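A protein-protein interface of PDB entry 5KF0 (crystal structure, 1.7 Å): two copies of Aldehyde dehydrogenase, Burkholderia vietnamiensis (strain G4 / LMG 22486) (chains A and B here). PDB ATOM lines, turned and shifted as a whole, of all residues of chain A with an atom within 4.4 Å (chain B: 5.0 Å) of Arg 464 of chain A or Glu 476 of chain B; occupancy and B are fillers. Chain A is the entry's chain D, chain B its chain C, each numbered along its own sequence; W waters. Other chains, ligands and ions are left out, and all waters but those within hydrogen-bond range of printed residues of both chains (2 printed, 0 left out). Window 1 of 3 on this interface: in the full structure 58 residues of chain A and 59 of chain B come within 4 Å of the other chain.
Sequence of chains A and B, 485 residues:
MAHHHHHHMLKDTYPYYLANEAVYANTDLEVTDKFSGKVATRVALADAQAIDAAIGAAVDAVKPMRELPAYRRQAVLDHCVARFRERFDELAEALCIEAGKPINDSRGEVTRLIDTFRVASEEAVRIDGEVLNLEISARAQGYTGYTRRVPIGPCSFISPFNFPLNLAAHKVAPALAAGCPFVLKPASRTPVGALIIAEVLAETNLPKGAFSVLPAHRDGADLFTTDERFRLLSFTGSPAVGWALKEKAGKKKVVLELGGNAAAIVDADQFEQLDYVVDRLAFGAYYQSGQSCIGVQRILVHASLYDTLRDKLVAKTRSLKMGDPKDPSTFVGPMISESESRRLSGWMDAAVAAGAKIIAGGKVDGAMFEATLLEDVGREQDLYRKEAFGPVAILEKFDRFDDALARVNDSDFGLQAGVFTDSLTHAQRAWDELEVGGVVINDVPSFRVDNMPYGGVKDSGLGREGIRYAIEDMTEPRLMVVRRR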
ATOM      1  N   GLU A 257     -22.057 -16.551  11.434  1.00  0.00           N
ATOM      2  CA  GLU A 257     -21.002 -15.991  10.586  1.00  0.00           C
ATOM      3  C   GLU A 257     -19.859 -15.629  11.523  1.00  0.00           C
ATOM      4  O   GLU A 257     -19.928 -14.612  12.222  1.00  0.00           O
ATOM      5  CB  GLU A 257     -21.504 -14.771   9.819  1.00  0.00           C
ATOM      6  CG  GLU A 257     -22.399 -15.130   8.625  1.00  0.00           C
ATOM      7  CD  GLU A 257     -21.606 -15.658   7.434  1.00  0.00           C
ATOM      8  OE1 GLU A 257     -20.359 -15.652   7.472  1.00  0.00           O
ATOM      9  OE2 GLU A 257     -22.237 -16.065   6.435  1.00  0.00           O
ATOM     10  N   GLY A 437     -15.136 -22.414   3.614  1.00  0.00           N
ATOM     11  CA  GLY A 437     -16.301 -21.977   2.860  1.00  0.00           C
ATOM     12  C   GLY A 437     -15.954 -21.559   1.445  1.00  0.00           C
ATOM     13  O   GLY A 437     -16.657 -21.909   0.495  1.00  0.00           O
ATOM     14  N   TYR A 454     -21.181 -16.733   1.073  1.00  0.00           N
ATOM     15  CA  TYR A 454     -20.080 -16.365   1.960  1.00  0.00           C
ATOM     16  C   TYR A 454     -20.307 -16.922   3.356  1.00  0.00           C
ATOM     17  O   TYR A 454     -21.350 -16.680   3.963  1.00  0.00           O
ATOM     18  CB  TYR A 454     -19.916 -14.842   2.046  1.00  0.00           C
ATOM     19  CG  TYR A 454     -18.834 -14.435   3.032  1.00  0.00           C
ATOM     20  CD1 TYR A 454     -17.492 -14.506   2.669  1.00  0.00           C
ATOM     21  CD2 TYR A 454     -19.154 -13.997   4.314  1.00  0.00           C
ATOM     22  CE1 TYR A 454     -16.482 -14.157   3.565  1.00  0.00           C
ATOM     23  CE2 TYR A 454     -18.147 -13.626   5.220  1.00  0.00           C
ATOM     24  CZ  TYR A 454     -16.823 -13.703   4.829  1.00  0.00           C
ATOM     25  OH  TYR A 454     -15.824 -13.344   5.706  1.00  0.00           O
ATOM     26  N   GLY A 455     -19.331 -17.654   3.873  1.00  0.00           N
ATOM     27  CA  GLY A 455     -19.454 -18.139   5.234  1.00  0.00           C
ATOM     28  C   GLY A 455     -18.379 -19.160   5.527  1.00  0.00           C
ATOM     29  O   GLY A 455     -17.501 -19.421   4.711  1.00  0.00           O
ATOM     30  N   GLY A 456     -18.464 -19.721   6.729  1.00  0.00           N
ATOM     31  CA  GLY A 456     -17.439 -20.636   7.195  1.00  0.00           C
ATOM     32  C   GLY A 456     -17.941 -22.034   7.493  1.00  0.00           C
ATOM     33  O   GLY A 456     -19.141 -22.246   7.697  1.00  0.00           O
ATOM     34  N   VAL A 457     -17.016 -22.995   7.487  1.00  0.00           N
ATOM     35  CA  VAL A 457     -17.238 -24.337   8.017  1.00  0.00           C
ATOM     36  C   VAL A 457     -16.322 -24.502   9.224  1.00  0.00           C
ATOM     37  O   VAL A 457     -15.635 -23.551   9.617  1.00  0.00           O
ATOM     38  CB  VAL A 457     -17.000 -25.423   6.946  1.00  0.00           C
ATOM     39  CG1 VAL A 457     -17.994 -25.249   5.791  1.00  0.00           C
ATOM     40  CG2 VAL A 457     -15.557 -25.391   6.409  1.00  0.00           C
ATOM     41  N   GLY A 463     -23.825 -22.008   7.844  1.00  0.00           N
ATOM     42  CA  GLY A 463     -24.687 -21.343   6.876  1.00  0.00           C
ATOM     43  C   GLY A 463     -23.937 -20.327   6.027  1.00  0.00           C
ATOM     44  O   GLY A 463     -22.723 -20.131   6.152  1.00  0.00           O
ATOM     45  N   ARG A 464     -24.685 -19.668   5.137  1.00  0.00           N
ATOM     46  CA  ARG A 464     -24.098 -18.705   4.208  1.00  0.00           C
ATOM     47  C   ARG A 464     -24.902 -17.415   4.163  1.00  0.00           C
ATOM     48  O   ARG A 464     -26.139 -17.437   4.204  1.00  0.00           O
ATOM     49  CB  ARG A 464     -23.998 -19.271   2.779  1.00  0.00           C
ATOM     50  CG  ARG A 464     -23.081 -20.495   2.643  1.00  0.00           C
ATOM     51  CD  ARG A 464     -21.596 -20.173   2.859  1.00  0.00           C
ATOM     52  NE  ARG A 464     -20.815 -21.392   2.645  1.00  0.00           N
ATOM     53  CZ  ARG A 464     -20.671 -22.352   3.558  1.00  0.00           C
ATOM     54  NH1 ARG A 464     -21.205 -22.210   4.775  1.00  0.00           N
ATOM     55  NH2 ARG A 464     -19.988 -23.452   3.257  1.00  0.00           N
ATOM     56  N   GLU A 465     -24.193 -16.296   4.055  1.00  0.00           N
ATOM     57  CA  GLU A 465     -24.781 -15.024   3.661  1.00  0.00           C
ATOM     58  C   GLU A 465     -24.373 -14.705   2.221  1.00  0.00           C
ATOM     59  O   GLU A 465     -23.826 -15.556   1.506  1.00  0.00           O
ATOM     60  CB  GLU A 465     -24.396 -13.922   4.658  1.00  0.00           C
ATOM     61  CG  GLU A 465     -25.125 -14.113   5.997  1.00  0.00           C
ATOM     62  CD  GLU A 465     -24.958 -12.952   6.961  1.00  0.00           C
ATOM     63  OE1 GLU A 465     -23.959 -12.214   6.840  1.00  0.00           O
ATOM     64  OE2 GLU A 465     -25.843 -12.773   7.826  1.00  0.00           O
ATOM     65  N   TYR A 469     -28.621 -16.316  -0.472  1.00  0.00           N
ATOM     66  CA  TYR A 469     -28.492 -17.388   0.504  1.00  0.00           C
ATOM     67  C   TYR A 469     -29.118 -16.978   1.822  1.00  0.00           C
ATOM     68  O   TYR A 469     -29.734 -17.807   2.507  1.00  0.00           O
ATOM     69  CB  TYR A 469     -27.001 -17.762   0.615  1.00  0.00           C
ATOM     70  CG  TYR A 469     -26.445 -17.836  -0.786  1.00  0.00           C
ATOM     71  CD1 TYR A 469     -25.712 -16.775  -1.331  1.00  0.00           C
ATOM     72  CD2 TYR A 469     -26.767 -18.903  -1.622  1.00  0.00           C
ATOM     73  CE1 TYR A 469     -25.286 -16.805  -2.644  1.00  0.00           C
ATOM     74  CE2 TYR A 469     -26.339 -18.937  -2.935  1.00  0.00           C
ATOM     75  CZ  TYR A 469     -25.596 -17.895  -3.439  1.00  0.00           C
ATOM     76  OH  TYR A 469     -25.173 -17.931  -4.754  1.00  0.00           O
ATOM     77  N   ALA A 470     -29.043 -15.687   2.139  1.00  0.00           N
ATOM     78  CA  ALA A 470     -29.755 -15.162   3.297  1.00  0.00           C
ATOM     79  C   ALA A 470     -31.268 -15.233   3.095  1.00  0.00           C
ATOM     80  O   ALA A 470     -32.008 -15.556   4.032  1.00  0.00           O
ATOM     81  CB  ALA A 470     -29.302 -13.727   3.563  1.00  0.00           C
ATOM     82  N   ASP A 473     -32.425 -18.661   3.956  1.00  0.00           N
ATOM     83  CA  ASP A 473     -32.542 -18.921   5.386  1.00  0.00           C
ATOM     84  C   ASP A 473     -33.696 -18.156   6.017  1.00  0.00           C
ATOM     85  O   ASP A 473     -34.225 -18.596   7.045  1.00  0.00           O
ATOM     86  CB  ASP A 473     -31.240 -18.578   6.109  1.00  0.00           C
ATOM     87  CG  ASP A 473     -30.194 -19.647   5.938  1.00  0.00           C
ATOM     88  OD1 ASP A 473     -30.580 -20.818   5.703  1.00  0.00           O
ATOM     89  OD2 ASP A 473     -28.996 -19.316   6.038  1.00  0.00           O
ATOM     90  N   ARG B 148     -19.536 -25.886  -5.795  1.00  0.00           N
ATOM     91  CA  ARG B 148     -19.684 -27.334  -5.731  1.00  0.00           C
ATOM     92  C   ARG B 148     -20.290 -27.672  -4.376  1.00  0.00           C
ATOM     93  O   ARG B 148     -20.236 -26.872  -3.435  1.00  0.00           O
ATOM     94  CB  ARG B 148     -18.335 -28.051  -5.914  1.00  0.00           C
ATOM     95  CG  ARG B 148     -17.378 -27.805  -4.748  1.00  0.00           C
ATOM     96  CD  ARG B 148     -15.956 -28.252  -5.054  1.00  0.00           C
ATOM     97  NE  ARG B 148     -15.804 -29.709  -5.087  1.00  0.00           N
ATOM     98  CZ  ARG B 148     -14.654 -30.302  -5.359  1.00  0.00           C
ATOM     99  NH1 ARG B 148     -13.579 -29.557  -5.617  1.00  0.00           N
ATOM    100  NH2 ARG B 148     -14.575 -31.631  -5.364  1.00  0.00           N
ATOM    101  N   ARG B 149     -20.868 -28.871  -4.273  1.00  0.00           N
ATOM    102  CA  ARG B 149     -21.407 -29.355  -3.007  1.00  0.00           C
ATOM    103  C   ARG B 149     -20.481 -30.442  -2.480  1.00  0.00           C
ATOM    104  O   ARG B 149     -20.317 -31.483  -3.126  1.00  0.00           O
ATOM    105  CB  ARG B 149     -22.826 -29.900  -3.185  1.00  0.00           C
ATOM    106  CG  ARG B 149     -23.783 -28.951  -3.877  1.00  0.00           C
ATOM    107  CD  ARG B 149     -24.054 -27.713  -3.036  1.00  0.00           C
ATOM    108  NE  ARG B 149     -24.579 -28.026  -1.709  1.00  0.00           N
ATOM    109  CZ  ARG B 149     -25.143 -27.128  -0.910  1.00  0.00           C
ATOM    110  NH1 ARG B 149     -25.270 -25.867  -1.320  1.00  0.00           N
ATOM    111  NH2 ARG B 149     -25.585 -27.477   0.289  1.00  0.00           N
ATOM    112  N   VAL B 150     -19.876 -30.207  -1.319  1.00  0.00           N
ATOM    113  CA  VAL B 150     -18.935 -31.147  -0.706  1.00  0.00           C
ATOM    114  C   VAL B 150     -19.670 -31.925   0.381  1.00  0.00           C
ATOM    115  O   VAL B 150     -20.411 -31.309   1.156  1.00  0.00           O
ATOM    116  CB  VAL B 150     -17.718 -30.401  -0.129  1.00  0.00           C
ATOM    117  CG1 VAL B 150     -16.783 -31.348   0.594  1.00  0.00           C
ATOM    118  CG2 VAL B 150     -16.975 -29.652  -1.239  1.00  0.00           C
ATOM    119  N   PRO B 151     -19.493 -33.243   0.502  1.00  0.00           N
ATOM    120  CA  PRO B 151     -20.146 -33.969   1.602  1.00  0.00           C
ATOM    121  C   PRO B 151     -19.841 -33.314   2.944  1.00  0.00           C
ATOM    122  O   PRO B 151     -18.717 -32.886   3.209  1.00  0.00           O
ATOM    123  CB  PRO B 151     -19.547 -35.379   1.524  1.00  0.00           C
ATOM    124  CG  PRO B 151     -18.839 -35.477   0.230  1.00  0.00           C
ATOM    125  CD  PRO B 151     -18.646 -34.104  -0.343  1.00  0.00           C
ATOM    126  N   ILE B 152     -20.864 -33.216   3.797  1.00  0.00           N
ATOM    127  CA  ILE B 152     -20.693 -32.484   5.051  1.00  0.00           C
ATOM    128  C   ILE B 152     -19.765 -33.234   6.015  1.00  0.00           C
ATOM    129  O   ILE B 152     -19.124 -32.612   6.870  1.00  0.00           O
ATOM    130  CB  ILE B 152     -22.073 -32.192   5.682  1.00  0.00           C
ATOM    131  CG1 ILE B 152     -21.974 -31.076   6.734  1.00  0.00           C
ATOM    132  CG2 ILE B 152     -22.684 -33.463   6.275  1.00  0.00           C
ATOM    133  CD1 ILE B 152     -23.333 -30.576   7.222  1.00  0.00           C
ATOM    134  N   MET B 474     -26.895 -32.400   3.580  1.00  0.00           N
ATOM    135  CA  MET B 474     -25.755 -33.282   3.791  1.00  0.00           C
ATOM    136  C   MET B 474     -24.521 -32.824   3.031  1.00  0.00           C
ATOM    137  O   MET B 474     -23.558 -33.588   2.915  1.00  0.00           O
ATOM    138  CB  MET B 474     -26.120 -34.709   3.388  1.00  0.00           C
ATOM    139  CG  MET B 474     -27.256 -35.268   4.229  1.00  0.00           C
ATOM    140  SD  MET B 474     -27.820 -36.895   3.701  1.00  0.00           S
ATOM    141  CE  MET B 474     -29.314 -37.058   4.687  1.00  0.00           C
ATOM    142  N   THR B 475     -24.541 -31.608   2.486  1.00  0.00           N
ATOM    143  CA  THR B 475     -23.383 -31.047   1.818  1.00  0.00           C
ATOM    144  C   THR B 475     -23.172 -29.617   2.294  1.00  0.00           C
ATOM    145  O   THR B 475     -24.106 -28.937   2.743  1.00  0.00           O
ATOM    146  CB  THR B 475     -23.532 -31.065   0.270  1.00  0.00           C
ATOM    147  OG1 THR B 475     -24.774 -30.458  -0.115  1.00  0.00           O
ATOM    148  CG2 THR B 475     -23.490 -32.507  -0.253  1.00  0.00           C
ATOM    149  N   GLU B 476     -21.925 -29.171   2.180  1.00  0.00           N
ATOM    150  CA  GLU B 476     -21.555 -27.775   2.329  1.00  0.00           C
ATOM    151  C   GLU B 476     -21.209 -27.212   0.967  1.00  0.00           C
ATOM    152  O   GLU B 476     -20.444 -27.839   0.220  1.00  0.00           O
ATOM    153  CB  GLU B 476     -20.343 -27.624   3.255  1.00  0.00           C
ATOM    154  CG  GLU B 476     -20.647 -27.770   4.738  1.00  0.00           C
ATOM    155  CD  GLU B 476     -21.284 -26.526   5.338  1.00  0.00           C
ATOM    156  OE1 GLU B 476     -21.585 -26.539   6.555  1.00  0.00           O
ATOM    157  OE2 GLU B 476     -21.485 -25.533   4.605  1.00  0.00           O
ATOM    158  N   PRO B 477     -21.718 -26.044   0.606  1.00  0.00           N
ATOM    159  CA  PRO B 477     -21.221 -25.398  -0.611  1.00  0.00           C
ATOM    160  C   PRO B 477     -19.779 -24.977  -0.402  1.00  0.00           C
ATOM    161  O   PRO B 477     -19.387 -24.537   0.686  1.00  0.00           O
ATOM    162  CB  PRO B 477     -22.152 -24.194  -0.788  1.00  0.00           C
ATOM    163  CG  PRO B 477     -22.685 -23.919   0.575  1.00  0.00           C
ATOM    164  CD  PRO B 477     -22.708 -25.224   1.326  1.00  0.00           C
ATOM    165  N   ARG B 478     -18.965 -25.153  -1.438  1.00  0.00           N
ATOM    166  CA  ARG B 478     -17.600 -24.642  -1.398  1.00  0.00           C
ATOM    167  C   ARG B 478     -17.399 -23.796  -2.643  1.00  0.00           C
ATOM    168  O   ARG B 478     -17.405 -24.318  -3.763  1.00  0.00           O
ATOM    169  CB  ARG B 478     -16.558 -25.763  -1.317  1.00  0.00           C
ATOM    170  CG  ARG B 478     -15.161 -25.216  -0.991  1.00  0.00           C
ATOM    171  CD  ARG B 478     -14.158 -26.354  -0.791  1.00  0.00           C
ATOM    172  NE  ARG B 478     -14.459 -27.112   0.428  1.00  0.00           N
ATOM    173  CZ  ARG B 478     -13.960 -28.315   0.714  1.00  0.00           C
ATOM    174  NH1 ARG B 478     -13.147 -28.925  -0.143  1.00  0.00           N
ATOM    175  NH2 ARG B 478     -14.276 -28.914   1.857  1.00  0.00           N
HETATM  176  O   HOH W   1     -19.519 -21.536   0.118  1.00  0.00           O
HETATM  177  O   HOH W   2     -21.463 -23.726   7.241  1.00  0.00           O
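The side-chain carboxylate (OE2) of Glu 476 of chain B lies within salt-bridge range of the guanidinium group (NH2) of Arg 464 of chain A (2.9 Å). The backbone carbonyl oxygen of Pro 477 of chain B lies within hydrogen-bond range of the guanidinium group of Arg 464 of chain A, 2.9 Å away.
N of Arg 478 of chain B sits at hydrogen-bond distance from O of Arg 148 of chain B, 2.9 Å away. The backbone NH of Glu 476 of chain B is in hydrogen-bond range of the backbone carbonyl oxygen of Val 150 of chain B (2.8 Å).
Pro 477 of chain B touches Gly 437 of chain A (O to O, 3.8 Å). Arg 478 of chain B touches Gly 437 of chain A. CD of Glu 476 of chain B touches CG1 of Val 457 of chain A (3.6 Å).
Of the printed residues of chain B, Gly 437 of chain A touches Pro 477 (3.8 Å) and Arg 478 (3.5 Å). Gly 455 of chain A touches none of the printed residues of chain B. Of the printed residues of chain B, Val 457 of chain A touches Glu 476 (3.6 Å). Of chain B, only Glu 476 and Pro 477 come within 4 Å of Arg 464 of chain A. Met 474 of chain B touches none of the printed residues of chain A. Of chain A, only Val 457 and Arg 464 come within 4 Å of Glu 476 of chain B. Of the printed residues of chain A, Pro 477 of chain B touches Gly 437 and Arg 464. Printed residues of chain A within 4 Å of Arg 478 of chain B: Gly 437. The nearest printed residue of chain B that does not touch Arg 464 of chain A is Arg 478 of chain B (5.1 Å).
Of the 12 printed residues of chain A, 3 touch a printed residue of chain B. Printed residues of chain A that touch a printed residue of chain B: Gly 437, Val 457 and Arg 464. Among the printed residues, Asp or Glu carboxylates within 4 Å of a Lys or Arg side-chain nitrogen of the other chain: Arg 464 of chain A with Glu 476 of chain B.
No position is printed for both chains. Of the 5 pairs that touch across the chains among the printed residues, none has its exchanged pair printed and touching as well.
Water W2 lies within hydrogen-bond range of O of Gly 456 of chain A, OE1 of Glu 476 of chain B, NH1 of Arg 464 of chain A and N of Gly 463 of chain A. Water W1 lies within hydrogen-bond range of the guanidinium group of Arg 464 of chain A (2.8 Å), the backbone carbonyl oxygen of Gly 437 of chain A (2.9 Å) and the backbone carbonyl oxygen of Pro 477 of chain B (3.1 Å).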
